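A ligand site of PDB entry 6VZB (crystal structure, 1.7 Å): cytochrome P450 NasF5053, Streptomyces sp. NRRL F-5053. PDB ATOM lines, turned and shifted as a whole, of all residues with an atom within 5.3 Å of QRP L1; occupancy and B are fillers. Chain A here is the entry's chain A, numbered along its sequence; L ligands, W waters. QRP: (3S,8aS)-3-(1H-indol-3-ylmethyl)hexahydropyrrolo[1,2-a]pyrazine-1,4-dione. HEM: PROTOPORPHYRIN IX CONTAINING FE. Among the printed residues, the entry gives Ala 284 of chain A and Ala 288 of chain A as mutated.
Water W1 lies within hydrogen-bond range of OE2 of Glu 314 (2.6 Å), NE1 of QRP L1 (2.8 Å) and N of Ala 284 (3.4 Å). Water W4 lies within hydrogen-bond range of an oxygen (O1A) of HEM L2 (2.6 Å), an oxygen (O) of QRP L1 (2.8 Å) and the backbone NH (N) of Lys 289 (3.0 Å). Water W2 lies within hydrogen-bond range of the side-chain carboxylate (OE1) of Glu 314 (2.7 Å), the backbone carbonyl oxygen (O) of Gly 286 (2.9 Å) and the backbone NH (N) of Leu 313 (3.0 Å).
Gln 72 touches QRP L1 (OE1 to CAI, 3.7 Å). OE1 of Glu 73 touches CAH of QRP L1 (3.5 Å). Thr 241 touches QRP L1 (CG2 to CH2, 3.7 Å). CD2 of Leu 283 touches CZ2 of QRP L1, 3.96 Å away. Ala 284 touches QRP L1. Ser 287 touches QRP L1. CA of Ala 288 touches CB of QRP L1, 3.6 Å away. Leu 313 touches QRP L1 (CD1 to NE1, 3.4 Å). Phe 387 touches QRP L1. Phe 388 touches QRP L1. Of the 17 residues printed, 12 come within 4 Å of QRP L1.
O2D of HEM L2 is in hydrogen-bond range of N of QRP L3 (3.0 Å).
The side-chain carboxylate of Glu 314 sits at hydrogen-bond distance from the backbone NH of Leu 283. N of Ala 284 is in hydrogen-bond range of OE2 of Glu 314, 3.2 Å away. N of Thr 285 is in hydrogen-bond range of O of Phe 387 (2.7 Å). The backbone NH (N) of Ser 287 lies within hydrogen-bond range of the side-chain amide oxygen (OE1) of Gln 72, 2.9 Å away.
O of QRP L1 lies within hydrogen-bond range of NZ of Lys 289 (3.0 Å). N of Gly 286 sits at hydrogen-bond distance from OAA of QRP L1, 3.0 Å away. O of QRP L3 sits at hydrogen-bond distance from NZ of Lys 289 (2.6 Å).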
ATOM      1  N   GLN A  72     -12.524 -20.287 -16.944  1.00  0.00           N
ATOM      2  CA  GLN A  72     -13.798 -20.874 -17.329  1.00  0.00           C
ATOM      3  C   GLN A  72     -14.976 -20.086 -16.759  1.00  0.00           C
ATOM      4  O   GLN A  72     -16.047 -20.079 -17.376  1.00  0.00           O
ATOM      5  CB  GLN A  72     -13.866 -22.333 -16.853  1.00  0.00           C
ATOM      6  CG  GLN A  72     -13.901 -22.459 -15.327  1.00  0.00           C
ATOM      7  CD  GLN A  72     -13.519 -23.810 -14.826  1.00  0.00           C
ATOM      8  OE1 GLN A  72     -14.314 -24.760 -14.852  1.00  0.00           O
ATOM      9  NE2 GLN A  72     -12.306 -23.914 -14.325  1.00  0.00           N
ATOM     10  N   GLU A  73     -14.825 -19.427 -15.606  1.00  0.00           N
ATOM     11  CA  GLU A  73     -15.946 -18.774 -14.948  1.00  0.00           C
ATOM     12  C   GLU A  73     -16.222 -17.410 -15.588  1.00  0.00           C
ATOM     13  O   GLU A  73     -15.318 -16.766 -16.114  1.00  0.00           O
ATOM     14  CB  GLU A  73     -15.671 -18.633 -13.436  1.00  0.00           C
ATOM     15  CG  GLU A  73     -14.473 -17.769 -13.004  1.00  0.00           C
ATOM     16  CD  GLU A  73     -13.149 -18.520 -12.929  1.00  0.00           C
ATOM     17  OE1 GLU A  73     -13.013 -19.557 -13.612  1.00  0.00           O
ATOM     18  OE2 GLU A  73     -12.239 -18.062 -12.207  1.00  0.00           O
ATOM     19  N   LEU A  77     -13.790 -14.533  -9.288  1.00  0.00           N
ATOM     20  CA  LEU A  77     -14.325 -15.084  -8.026  1.00  0.00           C
ATOM     21  C   LEU A  77     -13.743 -14.361  -6.817  1.00  0.00           C
ATOM     22  O   LEU A  77     -13.134 -14.956  -5.930  1.00  0.00           O
ATOM     23  CB  LEU A  77     -14.024 -16.570  -7.950  1.00  0.00           C
ATOM     24  CG  LEU A  77     -14.602 -17.380  -9.111  1.00  0.00           C
ATOM     25  CD1 LEU A  77     -14.248 -18.844  -8.884  1.00  0.00           C
ATOM     26  CD2 LEU A  77     -16.077 -17.192  -9.262  1.00  0.00           C
ATOM     27  N   PHE A 174     -22.019 -20.489 -13.517  1.00  0.00           N
ATOM     28  CA  PHE A 174     -21.666 -20.289 -14.911  1.00  0.00           C
ATOM     29  C   PHE A 174     -22.671 -19.446 -15.671  1.00  0.00           C
ATOM     30  O   PHE A 174     -22.313 -18.821 -16.677  1.00  0.00           O
ATOM     31  CB  PHE A 174     -21.555 -21.650 -15.600  1.00  0.00           C
ATOM     32  CG  PHE A 174     -20.273 -22.369 -15.313  1.00  0.00           C
ATOM     33  CD1 PHE A 174     -19.098 -21.941 -15.868  1.00  0.00           C
ATOM     34  CD2 PHE A 174     -20.255 -23.511 -14.526  1.00  0.00           C
ATOM     35  CE1 PHE A 174     -17.941 -22.584 -15.636  1.00  0.00           C
ATOM     36  CE2 PHE A 174     -19.081 -24.171 -14.296  1.00  0.00           C
ATOM     37  CZ  PHE A 174     -17.913 -23.717 -14.845  1.00  0.00           C
ATOM     38  N   THR A 241     -20.262 -26.522  -1.433  1.00  0.00           N
ATOM     39  CA  THR A 241     -19.633 -27.812  -1.662  1.00  0.00           C
ATOM     40  C   THR A 241     -20.252 -28.886  -0.764  1.00  0.00           C
ATOM     41  O   THR A 241     -20.720 -29.927  -1.252  1.00  0.00           O
ATOM     42  CB  THR A 241     -18.137 -27.677  -1.420  1.00  0.00           C
ATOM     43  OG1 THR A 241     -17.950 -27.099  -0.117  1.00  0.00           O
ATOM     44  CG2 THR A 241     -17.469 -26.767  -2.452  1.00  0.00           C
ATOM     45  N   LEU A 283     -19.940 -33.530  -8.358  1.00  0.00           N
ATOM     46  CA  LEU A 283     -20.188 -32.284  -7.640  1.00  0.00           C
ATOM     47  C   LEU A 283     -19.973 -31.096  -8.549  1.00  0.00           C
ATOM     48  O   LEU A 283     -20.945 -30.435  -8.942  1.00  0.00           O
ATOM     49  CB  LEU A 283     -19.305 -32.162  -6.405  1.00  0.00           C
ATOM     50  CG  LEU A 283     -19.526 -30.959  -5.489  1.00  0.00           C
ATOM     51  CD1 LEU A 283     -20.921 -30.882  -4.960  1.00  0.00           C
ATOM     52  CD2 LEU A 283     -18.596 -31.026  -4.322  1.00  0.00           C
ATOM     53  N   ALA A 284     -18.718 -30.789  -8.869  1.00  0.00           N
ATOM     54  CA  ALA A 284     -18.452 -29.591  -9.644  1.00  0.00           C
ATOM     55  C   ALA A 284     -18.900 -29.776 -11.088  1.00  0.00           C
ATOM     56  O   ALA A 284     -18.742 -30.846 -11.677  1.00  0.00           O
ATOM     57  CB  ALA A 284     -16.971 -29.254  -9.589  1.00  0.00           C
ATOM     58  N   THR A 285     -19.471 -28.728 -11.658  1.00  0.00           N
ATOM     59  CA  THR A 285     -19.793 -28.711 -13.068  1.00  0.00           C
ATOM     60  C   THR A 285     -18.708 -28.056 -13.908  1.00  0.00           C
ATOM     61  O   THR A 285     -18.781 -28.102 -15.149  1.00  0.00           O
ATOM     62  CB  THR A 285     -21.109 -27.948 -13.275  1.00  0.00           C
ATOM     63  OG1 THR A 285     -20.922 -26.595 -12.810  1.00  0.00           O
ATOM     64  CG2 THR A 285     -22.209 -28.598 -12.474  1.00  0.00           C
ATOM     65  N   GLY A 286     -17.737 -27.416 -13.268  1.00  0.00           N
ATOM     66  CA  GLY A 286     -16.511 -27.002 -13.891  1.00  0.00           C
ATOM     67  C   GLY A 286     -15.377 -27.943 -13.524  1.00  0.00           C
ATOM     68  O   GLY A 286     -15.580 -29.115 -13.200  1.00  0.00           O
ATOM     69  N   SER A 287     -14.163 -27.411 -13.583  1.00  0.00           N
ATOM     70  CA  SER A 287     -12.943 -28.203 -13.496  1.00  0.00           C
ATOM     71  C   SER A 287     -11.952 -27.534 -12.561  1.00  0.00           C
ATOM     72  O   SER A 287     -11.853 -26.314 -12.509  1.00  0.00           O
ATOM     73  CB  SER A 287     -12.269 -28.351 -14.858  1.00  0.00           C
ATOM     74  OG  SER A 287     -12.951 -29.289 -15.668  1.00  0.00           O
ATOM     75  N   ALA A 288     -11.201 -28.340 -11.820  1.00  0.00           N
ATOM     76  CA  ALA A 288      -9.990 -27.810 -11.219  1.00  0.00           C
ATOM     77  C   ALA A 288      -9.056 -27.349 -12.327  1.00  0.00           C
ATOM     78  O   ALA A 288      -9.092 -27.888 -13.438  1.00  0.00           O
ATOM     79  CB  ALA A 288      -9.328 -28.869 -10.357  1.00  0.00           C
ATOM     80  N   LYS A 289      -8.241 -26.339 -12.040  1.00  0.00           N
ATOM     81  CA  LYS A 289      -7.407 -25.830 -13.125  1.00  0.00           C
ATOM     82  C   LYS A 289      -6.086 -25.266 -12.593  1.00  0.00           C
ATOM     83  O   LYS A 289      -5.955 -24.903 -11.429  1.00  0.00           O
ATOM     84  CB  LYS A 289      -8.180 -24.779 -13.960  1.00  0.00           C
ATOM     85  CG  LYS A 289      -8.290 -23.392 -13.375  1.00  0.00           C
ATOM     86  CD  LYS A 289      -8.957 -23.396 -12.031  1.00  0.00           C
ATOM     87  CE  LYS A 289      -9.362 -21.998 -11.613  1.00  0.00           C
ATOM     88  NZ  LYS A 289      -9.783 -22.014 -10.181  1.00  0.00           N
ATOM     89  N   LEU A 313     -12.668 -33.368 -12.389  1.00  0.00           N
ATOM     90  CA  LEU A 313     -12.533 -34.435 -11.408  1.00  0.00           C
ATOM     91  C   LEU A 313     -13.614 -35.487 -11.597  1.00  0.00           C
ATOM     92  O   LEU A 313     -13.371 -36.691 -11.382  1.00  0.00           O
ATOM     93  CB  LEU A 313     -12.569 -33.833 -10.007  1.00  0.00           C
ATOM     94  CG  LEU A 313     -11.573 -32.696  -9.772  1.00  0.00           C
ATOM     95  CD1 LEU A 313     -11.622 -32.254  -8.320  1.00  0.00           C
ATOM     96  CD2 LEU A 313     -10.146 -33.142 -10.183  1.00  0.00           C
ATOM     97  N   GLU A 314     -14.802 -35.054 -12.023  1.00  0.00           N
ATOM     98  CA  GLU A 314     -15.856 -36.001 -12.385  1.00  0.00           C
ATOM     99  C   GLU A 314     -15.397 -36.922 -13.513  1.00  0.00           C
ATOM    100  O   GLU A 314     -15.643 -38.122 -13.482  1.00  0.00           O
ATOM    101  CB  GLU A 314     -17.111 -35.233 -12.806  1.00  0.00           C
ATOM    102  CG  GLU A 314     -17.850 -34.606 -11.672  1.00  0.00           C
ATOM    103  CD  GLU A 314     -17.068 -33.584 -10.903  1.00  0.00           C
ATOM    104  OE1 GLU A 314     -16.285 -32.809 -11.510  1.00  0.00           O
ATOM    105  OE2 GLU A 314     -17.273 -33.523  -9.675  1.00  0.00           O
ATOM    106  N   GLY A 340     -12.182 -37.043  -5.680  1.00  0.00           N
ATOM    107  CA  GLY A 340     -13.253 -36.171  -5.201  1.00  0.00           C
ATOM    108  C   GLY A 340     -12.767 -35.041  -4.326  1.00  0.00           C
ATOM    109  O   GLY A 340     -13.492 -34.064  -4.165  1.00  0.00           O
ATOM    110  N   PHE A 387     -21.739 -23.951  -9.958  1.00  0.00           N
ATOM    111  CA  PHE A 387     -20.505 -24.720  -9.973  1.00  0.00           C
ATOM    112  C   PHE A 387     -20.699 -26.048  -9.260  1.00  0.00           C
ATOM    113  O   PHE A 387     -20.150 -27.080  -9.674  1.00  0.00           O
ATOM    114  CB  PHE A 387     -19.374 -23.968  -9.264  1.00  0.00           C
ATOM    115  CG  PHE A 387     -18.921 -22.703  -9.940  1.00  0.00           C
ATOM    116  CD1 PHE A 387     -19.304 -22.356 -11.233  1.00  0.00           C
ATOM    117  CD2 PHE A 387     -18.081 -21.836  -9.239  1.00  0.00           C
ATOM    118  CE1 PHE A 387     -18.822 -21.168 -11.810  1.00  0.00           C
ATOM    119  CE2 PHE A 387     -17.626 -20.659  -9.806  1.00  0.00           C
ATOM    120  CZ  PHE A 387     -17.987 -20.331 -11.088  1.00  0.00           C
ATOM    121  N   PHE A 388     -21.412 -26.034  -8.132  1.00  0.00           N
ATOM    122  CA  PHE A 388     -21.539 -27.204  -7.278  1.00  0.00           C
ATOM    123  C   PHE A 388     -22.981 -27.662  -7.351  1.00  0.00           C
ATOM    124  O   PHE A 388     -23.887 -27.013  -6.792  1.00  0.00           O
ATOM    125  CB  PHE A 388     -21.051 -26.861  -5.873  1.00  0.00           C
ATOM    126  CG  PHE A 388     -19.619 -26.339  -5.857  1.00  0.00           C
ATOM    127  CD1 PHE A 388     -18.609 -27.118  -6.383  1.00  0.00           C
ATOM    128  CD2 PHE A 388     -19.311 -25.065  -5.420  1.00  0.00           C
ATOM    129  CE1 PHE A 388     -17.316 -26.654  -6.413  1.00  0.00           C
ATOM    130  CE2 PHE A 388     -18.017 -24.601  -5.450  1.00  0.00           C
ATOM    131  CZ  PHE A 388     -17.019 -25.396  -5.928  1.00  0.00           C
HETATM  132  C   QRP L   1     -12.718 -24.539  -9.602  1.00  0.00           C
HETATM  133  N   QRP L   1     -14.459 -26.311  -9.730  1.00  0.00           N
HETATM  134  O   QRP L   1     -11.559 -24.295  -9.542  1.00  0.00           O
HETATM  135  CA  QRP L   1     -13.390 -25.711  -8.973  1.00  0.00           C
HETATM  136  CB  QRP L   1     -12.320 -26.823  -8.690  1.00  0.00           C
HETATM  137  CG  QRP L   1     -13.119 -27.993  -8.004  1.00  0.00           C
HETATM  138  OAA QRP L   1     -16.295 -25.936 -11.053  1.00  0.00           O
HETATM  139  CAH QRP L   1     -14.607 -21.961 -11.600  1.00  0.00           C
HETATM  140  CAI QRP L   1     -15.497 -23.249 -11.652  1.00  0.00           C
HETATM  141  CAJ QRP L   1     -13.364 -22.352 -11.097  1.00  0.00           C
HETATM  142  CAN QRP L   1     -15.378 -25.502 -10.436  1.00  0.00           C
HETATM  143  CAT QRP L   1     -15.002 -23.995 -10.336  1.00  0.00           C
HETATM  144  NAU QRP L   1     -13.648 -23.690 -10.298  1.00  0.00           N
HETATM  145  CD1 QRP L   1     -13.369 -29.139  -8.728  1.00  0.00           C
HETATM  146  CD2 QRP L   1     -13.752 -28.096  -6.801  1.00  0.00           C
HETATM  147  NE1 QRP L   1     -14.142 -29.974  -7.958  1.00  0.00           N
HETATM  148  CE2 QRP L   1     -14.379 -29.317  -6.762  1.00  0.00           C
HETATM  149  CE3 QRP L   1     -13.820 -27.210  -5.714  1.00  0.00           C
HETATM  150  CH2 QRP L   1     -15.170 -28.801  -4.538  1.00  0.00           C
HETATM  151  CZ2 QRP L   1     -15.109 -29.660  -5.617  1.00  0.00           C
HETATM  152  CZ3 QRP L   1     -14.528 -27.560  -4.579  1.00  0.00           C
HETATM  153  CHA HEM L   2     -10.128 -27.484  -2.243  1.00  0.00           C
HETATM  154  CHB HEM L   2     -13.631 -30.815  -2.622  1.00  0.00           C
HETATM  155  CHC HEM L   2     -15.500 -29.361   1.571  1.00  0.00           C
HETATM  156  CHD HEM L   2     -11.903 -26.214   2.093  1.00  0.00           C
HETATM  157  C1A HEM L   2     -10.872 -28.549  -2.680  1.00  0.00           C
HETATM  158  C2A HEM L   2     -10.648 -29.305  -3.893  1.00  0.00           C
HETATM  159  C3A HEM L   2     -11.620 -30.223  -3.976  1.00  0.00           C
HETATM  160  C4A HEM L   2     -12.507 -30.070  -2.845  1.00  0.00           C
HETATM  161  CMA HEM L   2     -11.806 -31.265  -5.093  1.00  0.00           C
HETATM  162  CAA HEM L   2      -9.463 -29.149  -4.858  1.00  0.00           C
HETATM  163  CBA HEM L   2      -9.635 -28.057  -5.891  1.00  0.00           C
HETATM  164  CGA HEM L   2      -8.394 -27.945  -6.769  1.00  0.00           C
HETATM  165  O1A HEM L   2      -8.111 -26.812  -7.268  1.00  0.00           O
HETATM  166  O2A HEM L   2      -7.665 -28.951  -7.020  1.00  0.00           O
HETATM  167  C1B HEM L   2     -14.459 -30.714  -1.544  1.00  0.00           C
HETATM  168  C2B HEM L   2     -15.656 -31.473  -1.318  1.00  0.00           C
HETATM  169  C3B HEM L   2     -16.165 -31.081  -0.162  1.00  0.00           C
HETATM  170  C4B HEM L   2     -15.340 -30.006   0.360  1.00  0.00           C
HETATM  171  CMB HEM L   2     -16.200 -32.602  -2.201  1.00  0.00           C
HETATM  172  CAB HEM L   2     -17.466 -31.676   0.434  1.00  0.00           C
HETATM  173  CBB HEM L   2     -17.913 -31.414   1.663  1.00  0.00           C
HETATM  174  C1C HEM L   2     -14.662 -28.429   2.106  1.00  0.00           C
HETATM  175  C2C HEM L   2     -14.814 -27.788   3.404  1.00  0.00           C
HETATM  176  C3C HEM L   2     -13.790 -26.948   3.524  1.00  0.00           C
HETATM  177  C4C HEM L   2     -12.984 -27.008   2.323  1.00  0.00           C
HETATM  178  CMC HEM L   2     -15.908 -28.107   4.426  1.00  0.00           C
HETATM  179  CAC HEM L   2     -13.374 -25.983   4.641  1.00  0.00           C
HETATM  180  CBC HEM L   2     -14.187 -25.687   5.618  1.00  0.00           C
HETATM  181  C1D HEM L   2     -11.186 -26.205   0.936  1.00  0.00           C
HETATM  182  C2D HEM L   2     -10.133 -25.284   0.598  1.00  0.00           C
HETATM  183  C3D HEM L   2      -9.656 -25.635  -0.609  1.00  0.00           C
HETATM  184  C4D HEM L   2     -10.364 -26.802  -1.052  1.00  0.00           C
HETATM  185  CMD HEM L   2      -9.711 -24.080   1.463  1.00  0.00           C
HETATM  186  CAD HEM L   2      -8.537 -24.930  -1.425  1.00  0.00           C
HETATM  187  CBD HEM L   2      -7.229 -25.681  -1.397  1.00  0.00           C
HETATM  188  CGD HEM L   2      -6.179 -25.044  -2.295  1.00  0.00           C
HETATM  189  O1D HEM L   2      -4.959 -25.109  -1.966  1.00  0.00           O
HETATM  190  O2D HEM L   2      -6.567 -24.453  -3.330  1.00  0.00           O
HETATM  191  NA  HEM L   2     -12.011 -29.032  -2.078  1.00  0.00           N
HETATM  192  NB  HEM L   2     -14.288 -29.805  -0.517  1.00  0.00           N
HETATM  193  NC  HEM L   2     -13.520 -27.948   1.478  1.00  0.00           N
HETATM  194  ND  HEM L   2     -11.318 -27.127  -0.085  1.00  0.00           N
HETATM  195 FE   HEM L   2     -12.686 -28.634  -0.206  1.00  0.00          FE
HETATM  196  C   QRP L   3      -9.875 -21.693  -6.488  1.00  0.00           C
HETATM  197  N   QRP L   3      -8.707 -22.748  -4.475  1.00  0.00           N
HETATM  198  O   QRP L   3     -10.189 -21.685  -7.651  1.00  0.00           O
HETATM  199  CA  QRP L   3      -9.092 -22.797  -5.848  1.00  0.00           C
HETATM  200  CB  QRP L   3     -10.027 -24.106  -5.993  1.00  0.00           C
HETATM  201  CG  QRP L   3     -11.390 -24.003  -5.204  1.00  0.00           C
HETATM  202  OAA QRP L   3      -8.809 -21.673  -2.446  1.00  0.00           O
HETATM  203  CAH QRP L   3     -12.101 -19.477  -4.681  1.00  0.00           C
HETATM  204  CAI QRP L   3     -11.380 -20.379  -3.567  1.00  0.00           C
HETATM  205  CAJ QRP L   3     -11.229 -19.372  -5.769  1.00  0.00           C
HETATM  206  CAN QRP L   3      -9.133 -21.716  -3.596  1.00  0.00           C
HETATM  207  CAT QRP L   3      -9.975 -20.575  -4.270  1.00  0.00           C
HETATM  208  NAU QRP L   3     -10.317 -20.645  -5.570  1.00  0.00           N
HETATM  209  CD1 QRP L   3     -11.494 -24.615  -3.959  1.00  0.00           C
HETATM  210  CD2 QRP L   3     -12.609 -23.425  -5.460  1.00  0.00           C
HETATM  211  NE1 QRP L   3     -12.760 -24.384  -3.473  1.00  0.00           N
HETATM  212  CE2 QRP L   3     -13.460 -23.644  -4.404  1.00  0.00           C
HETATM  213  CE3 QRP L   3     -13.067 -22.678  -6.561  1.00  0.00           C
HETATM  214  CH2 QRP L   3     -15.231 -22.404  -5.536  1.00  0.00           C
HETATM  215  CZ2 QRP L   3     -14.779 -23.150  -4.449  1.00  0.00           C
HETATM  216  CZ3 QRP L   3     -14.381 -22.197  -6.609  1.00  0.00           C
HETATM  217  O   HOH W   1     -15.736 -32.242  -8.000  1.00  0.00           O
HETATM  218  O   HOH W   2     -14.233 -31.015 -11.530  1.00  0.00           O
HETATM  219  O   HOH W   3     -13.807 -26.449  -1.517  1.00  0.00           O
HETATM  220  O   HOH W   4      -8.994 -25.399  -9.295  1.00  0.00           O
